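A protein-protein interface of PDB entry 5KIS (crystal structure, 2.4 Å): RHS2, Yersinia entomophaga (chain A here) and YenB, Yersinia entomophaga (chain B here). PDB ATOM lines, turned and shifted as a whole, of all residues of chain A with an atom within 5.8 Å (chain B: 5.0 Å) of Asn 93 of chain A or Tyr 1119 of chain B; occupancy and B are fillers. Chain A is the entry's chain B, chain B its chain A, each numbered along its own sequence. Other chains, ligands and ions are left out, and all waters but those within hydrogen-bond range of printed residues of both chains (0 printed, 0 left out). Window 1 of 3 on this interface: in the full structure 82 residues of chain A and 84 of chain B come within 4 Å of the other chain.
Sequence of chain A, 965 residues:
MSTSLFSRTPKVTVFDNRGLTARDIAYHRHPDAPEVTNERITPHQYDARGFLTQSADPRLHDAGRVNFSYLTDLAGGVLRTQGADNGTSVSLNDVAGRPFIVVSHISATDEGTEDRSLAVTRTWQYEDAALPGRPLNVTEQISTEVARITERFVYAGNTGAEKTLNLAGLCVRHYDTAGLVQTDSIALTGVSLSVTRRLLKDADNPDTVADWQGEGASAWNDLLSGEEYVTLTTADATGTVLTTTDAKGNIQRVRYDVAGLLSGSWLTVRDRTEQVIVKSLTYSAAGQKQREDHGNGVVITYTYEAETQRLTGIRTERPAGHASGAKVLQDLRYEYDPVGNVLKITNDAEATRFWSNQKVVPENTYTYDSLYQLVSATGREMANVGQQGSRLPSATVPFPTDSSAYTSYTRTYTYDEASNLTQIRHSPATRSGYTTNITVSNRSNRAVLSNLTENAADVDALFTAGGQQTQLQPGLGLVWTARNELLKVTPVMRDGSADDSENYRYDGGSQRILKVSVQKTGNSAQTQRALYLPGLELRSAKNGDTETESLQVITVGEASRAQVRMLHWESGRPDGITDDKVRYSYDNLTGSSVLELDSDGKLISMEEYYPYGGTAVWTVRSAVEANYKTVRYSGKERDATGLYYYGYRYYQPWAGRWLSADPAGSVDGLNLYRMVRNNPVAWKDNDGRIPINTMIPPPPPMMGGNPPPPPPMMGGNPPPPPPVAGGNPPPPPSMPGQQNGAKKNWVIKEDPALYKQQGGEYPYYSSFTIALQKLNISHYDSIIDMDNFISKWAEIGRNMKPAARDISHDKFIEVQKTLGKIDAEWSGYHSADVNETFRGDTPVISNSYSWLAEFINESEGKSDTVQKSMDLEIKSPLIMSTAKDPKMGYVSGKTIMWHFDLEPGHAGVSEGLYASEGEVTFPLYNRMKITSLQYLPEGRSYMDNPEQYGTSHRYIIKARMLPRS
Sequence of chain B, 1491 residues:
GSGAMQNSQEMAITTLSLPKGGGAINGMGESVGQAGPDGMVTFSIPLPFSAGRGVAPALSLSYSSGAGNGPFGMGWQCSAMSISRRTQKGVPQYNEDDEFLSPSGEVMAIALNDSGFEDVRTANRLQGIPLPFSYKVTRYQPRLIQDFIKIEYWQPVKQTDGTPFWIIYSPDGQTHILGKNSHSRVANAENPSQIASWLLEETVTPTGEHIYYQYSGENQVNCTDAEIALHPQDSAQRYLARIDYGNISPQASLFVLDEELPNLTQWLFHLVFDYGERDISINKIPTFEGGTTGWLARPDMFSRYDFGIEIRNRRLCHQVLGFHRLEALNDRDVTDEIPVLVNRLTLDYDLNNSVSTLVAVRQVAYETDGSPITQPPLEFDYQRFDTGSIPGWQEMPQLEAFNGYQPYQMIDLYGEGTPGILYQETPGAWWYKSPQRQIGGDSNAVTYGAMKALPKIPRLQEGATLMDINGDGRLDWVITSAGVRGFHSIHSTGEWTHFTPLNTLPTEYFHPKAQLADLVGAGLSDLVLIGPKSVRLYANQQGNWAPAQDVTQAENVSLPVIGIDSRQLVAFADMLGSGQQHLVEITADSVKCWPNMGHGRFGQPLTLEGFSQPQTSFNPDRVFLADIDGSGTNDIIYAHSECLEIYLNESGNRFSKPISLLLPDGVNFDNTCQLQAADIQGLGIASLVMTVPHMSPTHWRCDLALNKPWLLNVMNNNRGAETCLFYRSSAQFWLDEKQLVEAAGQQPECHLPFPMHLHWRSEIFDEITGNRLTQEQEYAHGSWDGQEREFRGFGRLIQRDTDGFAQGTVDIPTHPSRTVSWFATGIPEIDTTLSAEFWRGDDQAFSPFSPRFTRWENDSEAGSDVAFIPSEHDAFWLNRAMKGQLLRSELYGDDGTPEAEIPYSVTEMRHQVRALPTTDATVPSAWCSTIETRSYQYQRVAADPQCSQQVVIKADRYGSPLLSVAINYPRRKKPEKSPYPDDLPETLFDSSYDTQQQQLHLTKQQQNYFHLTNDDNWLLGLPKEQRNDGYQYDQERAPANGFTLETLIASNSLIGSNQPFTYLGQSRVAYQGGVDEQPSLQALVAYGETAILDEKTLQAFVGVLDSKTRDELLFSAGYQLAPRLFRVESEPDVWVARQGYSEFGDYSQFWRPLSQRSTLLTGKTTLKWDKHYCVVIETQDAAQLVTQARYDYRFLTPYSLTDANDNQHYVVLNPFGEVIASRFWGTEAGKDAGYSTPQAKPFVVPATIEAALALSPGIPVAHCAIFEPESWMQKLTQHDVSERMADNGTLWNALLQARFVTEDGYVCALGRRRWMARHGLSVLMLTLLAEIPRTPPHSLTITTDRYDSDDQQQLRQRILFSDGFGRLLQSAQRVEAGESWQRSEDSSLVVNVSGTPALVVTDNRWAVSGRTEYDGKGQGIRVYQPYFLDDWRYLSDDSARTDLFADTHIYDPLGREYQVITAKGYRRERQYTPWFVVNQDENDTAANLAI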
ATOM      1  N   ASP A  73     -20.973   9.078  20.074  1.00  0.00           N
ATOM      2  CA  ASP A  73     -20.025   9.288  21.160  1.00  0.00           C
ATOM      3  C   ASP A  73     -20.665  10.260  22.156  1.00  0.00           C
ATOM      4  O   ASP A  73     -21.776  10.736  21.944  1.00  0.00           O
ATOM      5  CB  ASP A  73     -18.627   9.713  20.638  1.00  0.00           C
ATOM      6  CG  ASP A  73     -18.583  11.117  20.037  1.00  0.00           C
ATOM      7  OD1 ASP A  73     -19.390  11.998  20.384  1.00  0.00           O
ATOM      8  OD2 ASP A  73     -17.685  11.344  19.206  1.00  0.00           O
ATOM      9  N   SER A  91     -17.984   5.198  11.604  1.00  0.00           N
ATOM     10  CA  SER A  91     -17.171   6.387  11.369  1.00  0.00           C
ATOM     11  C   SER A  91     -16.429   6.767  12.652  1.00  0.00           C
ATOM     12  O   SER A  91     -16.967   6.622  13.754  1.00  0.00           O
ATOM     13  CB  SER A  91     -18.078   7.536  10.927  1.00  0.00           C
ATOM     14  OG  SER A  91     -17.488   8.250   9.866  1.00  0.00           O
ATOM     15  N   LEU A  92     -15.187   7.226  12.513  1.00  0.00           N
ATOM     16  CA  LEU A  92     -14.416   7.748  13.646  1.00  0.00           C
ATOM     17  C   LEU A  92     -13.468   8.837  13.167  1.00  0.00           C
ATOM     18  O   LEU A  92     -12.631   8.595  12.297  1.00  0.00           O
ATOM     19  CB  LEU A  92     -13.627   6.632  14.341  1.00  0.00           C
ATOM     20  CG  LEU A  92     -12.763   7.060  15.539  1.00  0.00           C
ATOM     21  CD1 LEU A  92     -13.629   7.356  16.762  1.00  0.00           C
ATOM     22  CD2 LEU A  92     -11.701   6.014  15.854  1.00  0.00           C
ATOM     23  N   ASN A  93     -13.612  10.034  13.727  1.00  0.00           N
ATOM     24  CA  ASN A  93     -12.652  11.109  13.499  1.00  0.00           C
ATOM     25  C   ASN A  93     -11.606  11.097  14.603  1.00  0.00           C
ATOM     26  O   ASN A  93     -11.888  10.698  15.733  1.00  0.00           O
ATOM     27  CB  ASN A  93     -13.359  12.463  13.471  1.00  0.00           C
ATOM     28  CG  ASN A  93     -14.325  12.590  12.313  1.00  0.00           C
ATOM     29  OD1 ASN A  93     -14.030  12.187  11.192  1.00  0.00           O
ATOM     30  ND2 ASN A  93     -15.493  13.138  12.582  1.00  0.00           N
ATOM     31  N   ASP A  94     -10.398  11.537  14.281  1.00  0.00           N
ATOM     32  CA  ASP A  94      -9.369  11.660  15.300  1.00  0.00           C
ATOM     33  C   ASP A  94      -9.641  12.861  16.220  1.00  0.00           C
ATOM     34  O   ASP A  94     -10.552  13.650  15.979  1.00  0.00           O
ATOM     35  CB  ASP A  94      -7.943  11.645  14.691  1.00  0.00           C
ATOM     36  CG  ASP A  94      -7.637  12.821  13.752  1.00  0.00           C
ATOM     37  OD1 ASP A  94      -8.239  13.913  13.884  1.00  0.00           O
ATOM     38  OD2 ASP A  94      -6.733  12.633  12.890  1.00  0.00           O
ATOM     39  N   VAL A  95      -8.866  12.972  17.288  1.00  0.00           N
ATOM     40  CA  VAL A  95      -9.011  14.077  18.244  1.00  0.00           C
ATOM     41  C   VAL A  95      -8.843  15.479  17.633  1.00  0.00           C
ATOM     42  O   VAL A  95      -9.354  16.447  18.186  1.00  0.00           O
ATOM     43  CB  VAL A  95      -8.065  13.925  19.468  1.00  0.00           C
ATOM     44  CG1 VAL A  95      -8.431  12.685  20.266  1.00  0.00           C
ATOM     45  CG2 VAL A  95      -6.583  13.901  19.069  1.00  0.00           C
ATOM     46  N   GLY A  97     -10.364  16.295  14.947  1.00  0.00           N
ATOM     47  CA  GLY A  97     -11.591  16.480  14.162  1.00  0.00           C
ATOM     48  C   GLY A  97     -11.549  16.020  12.705  1.00  0.00           C
ATOM     49  O   GLY A  97     -12.516  16.221  11.972  1.00  0.00           O
ATOM     50  N   ARG A  98     -10.460  15.376  12.288  1.00  0.00           N
ATOM     51  CA  ARG A  98     -10.254  15.009  10.889  1.00  0.00           C
ATOM     52  C   ARG A  98     -10.823  13.598  10.649  1.00  0.00           C
ATOM     53  O   ARG A  98     -10.904  12.809  11.583  1.00  0.00           O
ATOM     54  CB  ARG A  98      -8.754  15.020  10.547  1.00  0.00           C
ATOM     55  CG  ARG A  98      -7.992  16.246  11.037  1.00  0.00           C
ATOM     56  CD  ARG A  98      -6.500  16.202  10.724  1.00  0.00           C
ATOM     57  NE  ARG A  98      -5.799  15.133  11.436  1.00  0.00           N
ATOM     58  CZ  ARG A  98      -4.480  15.064  11.622  1.00  0.00           C
ATOM     59  NH1 ARG A  98      -3.660  16.013  11.182  1.00  0.00           N
ATOM     60  NH2 ARG A  98      -3.972  14.028  12.274  1.00  0.00           N
ATOM     61  N   PRO A  99     -11.208  13.270   9.403  1.00  0.00           N
ATOM     62  CA  PRO A  99     -11.535  11.881   9.072  1.00  0.00           C
ATOM     63  C   PRO A  99     -10.381  10.935   9.382  1.00  0.00           C
ATOM     64  O   PRO A  99      -9.240  11.233   9.033  1.00  0.00           O
ATOM     65  CB  PRO A  99     -11.789  11.935   7.559  1.00  0.00           C
ATOM     66  CG  PRO A  99     -12.281  13.316   7.320  1.00  0.00           C
ATOM     67  CD  PRO A  99     -11.507  14.179   8.280  1.00  0.00           C
ATOM     68  N   PHE A 100     -10.674   9.832  10.066  1.00  0.00           N
ATOM     69  CA  PHE A 100      -9.659   8.810  10.368  1.00  0.00           C
ATOM     70  C   PHE A 100     -10.005   7.442   9.775  1.00  0.00           C
ATOM     71  O   PHE A 100      -9.148   6.782   9.197  1.00  0.00           O
ATOM     72  CB  PHE A 100      -9.445   8.682  11.881  1.00  0.00           C
ATOM     73  CG  PHE A 100      -8.225   7.898  12.243  1.00  0.00           C
ATOM     74  CD1 PHE A 100      -6.966   8.505  12.226  1.00  0.00           C
ATOM     75  CD2 PHE A 100      -8.320   6.554  12.571  1.00  0.00           C
ATOM     76  CE1 PHE A 100      -5.826   7.785  12.547  1.00  0.00           C
ATOM     77  CE2 PHE A 100      -7.184   5.828  12.886  1.00  0.00           C
ATOM     78  CZ  PHE A 100      -5.936   6.443  12.877  1.00  0.00           C
ATOM     79  N   ILE A 101     -11.246   7.009   9.948  1.00  0.00           N
ATOM     80  CA  ILE A 101     -11.696   5.748   9.386  1.00  0.00           C
ATOM     81  C   ILE A 101     -13.203   5.767   9.133  1.00  0.00           C
ATOM     82  O   ILE A 101     -13.965   6.356   9.897  1.00  0.00           O
ATOM     83  CB  ILE A 101     -11.291   4.561  10.291  1.00  0.00           C
ATOM     84  CG1 ILE A 101     -11.631   3.225   9.636  1.00  0.00           C
ATOM     85  CG2 ILE A 101     -11.939   4.667  11.664  1.00  0.00           C
ATOM     86  CD1 ILE A 101     -11.039   2.044  10.365  1.00  0.00           C
ATOM     87  N   ILE B1092     -14.910  11.126  25.546  1.00  0.00           N
ATOM     88  CA  ILE B1092     -15.499  10.888  24.236  1.00  0.00           C
ATOM     89  C   ILE B1092     -16.138   9.496  24.138  1.00  0.00           C
ATOM     90  O   ILE B1092     -17.186   9.354  23.496  1.00  0.00           O
ATOM     91  CB  ILE B1092     -14.440  11.106  23.120  1.00  0.00           C
ATOM     92  CG1 ILE B1092     -13.832  12.522  23.230  1.00  0.00           C
ATOM     93  CG2 ILE B1092     -15.022  10.851  21.728  1.00  0.00           C
ATOM     94  CD1 ILE B1092     -14.829  13.671  23.174  1.00  0.00           C
ATOM     95  N   LEU B1114      -7.982   3.631  18.295  1.00  0.00           N
ATOM     96  CA  LEU B1114      -8.276   4.756  19.190  1.00  0.00           C
ATOM     97  C   LEU B1114      -6.999   5.450  19.712  1.00  0.00           C
ATOM     98  O   LEU B1114      -6.973   6.691  19.799  1.00  0.00           O
ATOM     99  CB  LEU B1114      -9.200   4.325  20.340  1.00  0.00           C
ATOM    100  CG  LEU B1114     -10.654   3.986  19.959  1.00  0.00           C
ATOM    101  CD1 LEU B1114     -11.375   3.204  21.048  1.00  0.00           C
ATOM    102  CD2 LEU B1114     -11.455   5.236  19.623  1.00  0.00           C
ATOM    103  N   PHE B1115      -5.949   4.670  20.022  1.00  0.00           N
ATOM    104  CA  PHE B1115      -4.650   5.222  20.429  1.00  0.00           C
ATOM    105  C   PHE B1115      -4.008   6.026  19.279  1.00  0.00           C
ATOM    106  O   PHE B1115      -3.498   7.133  19.490  1.00  0.00           O
ATOM    107  CB  PHE B1115      -3.687   4.112  20.903  1.00  0.00           C
ATOM    108  CG  PHE B1115      -3.994   3.559  22.279  1.00  0.00           C
ATOM    109  CD1 PHE B1115      -4.065   4.395  23.386  1.00  0.00           C
ATOM    110  CD2 PHE B1115      -4.163   2.193  22.474  1.00  0.00           C
ATOM    111  CE1 PHE B1115      -4.329   3.882  24.651  1.00  0.00           C
ATOM    112  CE2 PHE B1115      -4.424   1.678  23.732  1.00  0.00           C
ATOM    113  CZ  PHE B1115      -4.508   2.522  24.822  1.00  0.00           C
ATOM    114  N   ALA B1117      -5.554   7.332  16.720  1.00  0.00           N
ATOM    115  CA  ALA B1117      -6.432   8.492  16.519  1.00  0.00           C
ATOM    116  C   ALA B1117      -6.216   9.611  17.558  1.00  0.00           C
ATOM    117  O   ALA B1117      -6.893  10.636  17.517  1.00  0.00           O
ATOM    118  CB  ALA B1117      -7.886   8.044  16.514  1.00  0.00           C
ATOM    119  N   GLY B1118      -5.295   9.416  18.499  1.00  0.00           N
ATOM    120  CA  GLY B1118      -4.929  10.453  19.451  1.00  0.00           C
ATOM    121  C   GLY B1118      -5.740  10.427  20.726  1.00  0.00           C
ATOM    122  O   GLY B1118      -5.501  11.249  21.600  1.00  0.00           O
ATOM    123  N   TYR B1119      -6.691   9.497  20.846  1.00  0.00           N
ATOM    124  CA  TYR B1119      -7.446   9.337  22.095  1.00  0.00           C
ATOM    125  C   TYR B1119      -6.576   8.617  23.123  1.00  0.00           C
ATOM    126  O   TYR B1119      -5.529   8.062  22.781  1.00  0.00           O
ATOM    127  CB  TYR B1119      -8.744   8.557  21.886  1.00  0.00           C
ATOM    128  CG  TYR B1119      -9.715   9.192  20.926  1.00  0.00           C
ATOM    129  CD1 TYR B1119     -10.598  10.191  21.341  1.00  0.00           C
ATOM    130  CD2 TYR B1119      -9.766   8.792  19.590  1.00  0.00           C
ATOM    131  CE1 TYR B1119     -11.497  10.773  20.451  1.00  0.00           C
ATOM    132  CE2 TYR B1119     -10.658   9.369  18.697  1.00  0.00           C
ATOM    133  CZ  TYR B1119     -11.520  10.356  19.135  1.00  0.00           C
ATOM    134  OH  TYR B1119     -12.390  10.917  18.247  1.00  0.00           O
ATOM    135  N   GLN B1120      -7.001   8.646  24.375  1.00  0.00           N
ATOM    136  CA  GLN B1120      -6.273   7.975  25.450  1.00  0.00           C
ATOM    137  C   GLN B1120      -7.185   7.663  26.623  1.00  0.00           C
ATOM    138  O   GLN B1120      -8.255   8.280  26.798  1.00  0.00           O
ATOM    139  CB  GLN B1120      -5.057   8.791  25.910  1.00  0.00           C
ATOM    140  CG  GLN B1120      -5.326  10.260  26.206  1.00  0.00           C
ATOM    141  CD  GLN B1120      -4.073  11.025  26.624  1.00  0.00           C
ATOM    142  OE1 GLN B1120      -3.627  11.936  25.933  1.00  0.00           O
ATOM    143  NE2 GLN B1120      -3.502  10.652  27.763  1.00  0.00           N
ATOM    144  N   LEU B1121      -6.765   6.671  27.402  1.00  0.00           N
ATOM    145  CA  LEU B1121      -7.495   6.278  28.596  1.00  0.00           C
ATOM    146  C   LEU B1121      -7.114   7.183  29.740  1.00  0.00           C
ATOM    147  O   LEU B1121      -5.931   7.465  29.963  1.00  0.00           O
ATOM    148  CB  LEU B1121      -7.222   4.827  28.961  1.00  0.00           C
ATOM    149  CG  LEU B1121      -7.914   3.843  28.019  1.00  0.00           C
ATOM    150  CD1 LEU B1121      -7.314   2.451  28.179  1.00  0.00           C
ATOM    151  CD2 LEU B1121      -9.424   3.832  28.241  1.00  0.00           C
ATOM    152  N   TRP B1135     -12.339   6.924  27.290  1.00  0.00           N
ATOM    153  CA  TRP B1135     -11.502   7.441  26.216  1.00  0.00           C
ATOM    154  C   TRP B1135     -11.690   8.938  26.137  1.00  0.00           C
ATOM    155  O   TRP B1135     -12.820   9.408  25.988  1.00  0.00           O
ATOM    156  CB  TRP B1135     -11.872   6.790  24.897  1.00  0.00           C
ATOM    157  CG  TRP B1135     -11.521   5.338  24.877  1.00  0.00           C
ATOM    158  CD1 TRP B1135     -12.324   4.290  25.207  1.00  0.00           C
ATOM    159  CD2 TRP B1135     -10.254   4.783  24.532  1.00  0.00           C
ATOM    160  NE1 TRP B1135     -11.636   3.107  25.068  1.00  0.00           N
ATOM    161  CE2 TRP B1135     -10.361   3.388  24.657  1.00  0.00           C
ATOM    162  CE3 TRP B1135      -9.037   5.334  24.121  1.00  0.00           C
ATOM    163  CZ2 TRP B1135      -9.305   2.536  24.383  1.00  0.00           C
ATOM    164  CZ3 TRP B1135      -7.984   4.488  23.848  1.00  0.00           C
ATOM    165  CH2 TRP B1135      -8.123   3.102  23.983  1.00  0.00           C
ATOM    166  N   VAL B1136     -10.586   9.678  26.239  1.00  0.00           N
ATOM    167  CA  VAL B1136     -10.642  11.137  26.264  1.00  0.00           C
ATOM    168  C   VAL B1136      -9.850  11.770  25.126  1.00  0.00           C
ATOM    169  O   VAL B1136      -8.902  11.182  24.606  1.00  0.00           O
ATOM    170  CB  VAL B1136     -10.150  11.706  27.612  1.00  0.00           C
ATOM    171  CG1 VAL B1136     -10.881  11.037  28.770  1.00  0.00           C
ATOM    172  CG2 VAL B1136      -8.634  11.577  27.769  1.00  0.00           C
ATOM    173  N   ALA B1137     -10.260  12.977  24.754  1.00  0.00           N
ATOM    174  CA  ALA B1137      -9.561  13.788  23.772  1.00  0.00           C
ATOM    175  C   ALA B1137      -9.026  15.010  24.481  1.00  0.00           C
ATOM    176  O   ALA B1137      -9.729  15.606  25.293  1.00  0.00           O
ATOM    177  CB  ALA B1137     -10.515  14.203  22.672  1.00  0.00           C
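The backbone carbonyl oxygen of Ala 1117 of chain B lies within hydrogen-bond range of the backbone NH of Val 95 of chain A (3.1 Å).
The side-chain hydroxyl of Tyr 1119 of chain B sits at hydrogen-bond distance from the backbone carbonyl oxygen of Asn 93 of chain A, 2.6 Å away.
O of Ile 1092 of chain B touches CB of Asp 73 of chain A (3.2 Å).
CD2 of Leu 92 of chain A touches CD2 of Leu 1114 of chain B, 3.9 Å away.
CB of Asp 94 of chain A touches O of Ala 1117 of chain B, 3.2 Å away.
Tyr 1119 of chain B touches Asp 94 of chain A.
Val 95 of chain A touches Gly 1118 of chain B (CG1 to O, 3.5 Å).
CG1 of Val 95 of chain A touches CD1 of Tyr 1119 of chain B (3.5 Å).
Ala 1137 of chain B touches Val 95 of chain A (CB to CG1, 3.5 Å).
CZ of Phe 100 of chain A touches N of Ala 1117 of chain B, at 3.96 Å.
The backbone carbonyl oxygen (O) of Trp 1135 of chain B sits at hydrogen-bond distance from the backbone NH (N) of Ile 1092 of chain B.
The backbone carbonyl oxygen (O) of Leu 1114 of chain B is in hydrogen-bond range of the backbone NH (N) of Tyr 1119 of chain B (3.0 Å).
The backbone carbonyl oxygen (O) of Ile 101 of chain A sits at hydrogen-bond distance from the backbone NH (N) of Leu 92 of chain A, at 3.0 Å.
The side-chain amide oxygen (OD1) of Asn 93 of chain A sits close to the backbone carbonyl oxygen (O) of Arg 98 of chain A, 3.2 Å away.
The backbone NH of Gly 97 of chain A is in hydrogen-bond range of the side-chain carboxylate of Asp 94 of chain A (3.4 Å).
The side-chain carboxylate (OD2) of Asp 94 of chain A is in salt-bridge range of the guanidinium group (NE) of Arg 98 of chain A (3.0 Å).
Ser 91 of chain A touches none of the printed residues of chain B.
Of chain B, only Tyr 1119 (2.6 Å) comes within 4 Å of Asn 93 of chain A.
Of the printed residues of chain B, Asp 94 of chain A touches Ala 1117 (3.2 Å) and Tyr 1119 (3.9 Å).
Of the printed residues of chain A, Leu 1114 of chain B touches Leu 92 (3.9 Å).
Tyr 1119 of chain B touches just these residues of chain A: Asn 93, Asp 94 and Val 95.
Val 1136 of chain B touches none of the printed residues of chain A.
The nearest residue of chain A that does not touch Tyr 1119 of chain B is Leu 92 of chain A (4.1 Å).
Of the 11 printed residues of chain A, 6 touch a printed residue of chain B.
Printed residues of chain A that touch a printed residue of chain B: Asp 73, Leu 92, Asn 93, Asp 94, Val 95 and Phe 100.
Among the printed residues, no Asp or Glu carboxylate lies within 4 Å of a Lys or Arg side-chain nitrogen of the other chain.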
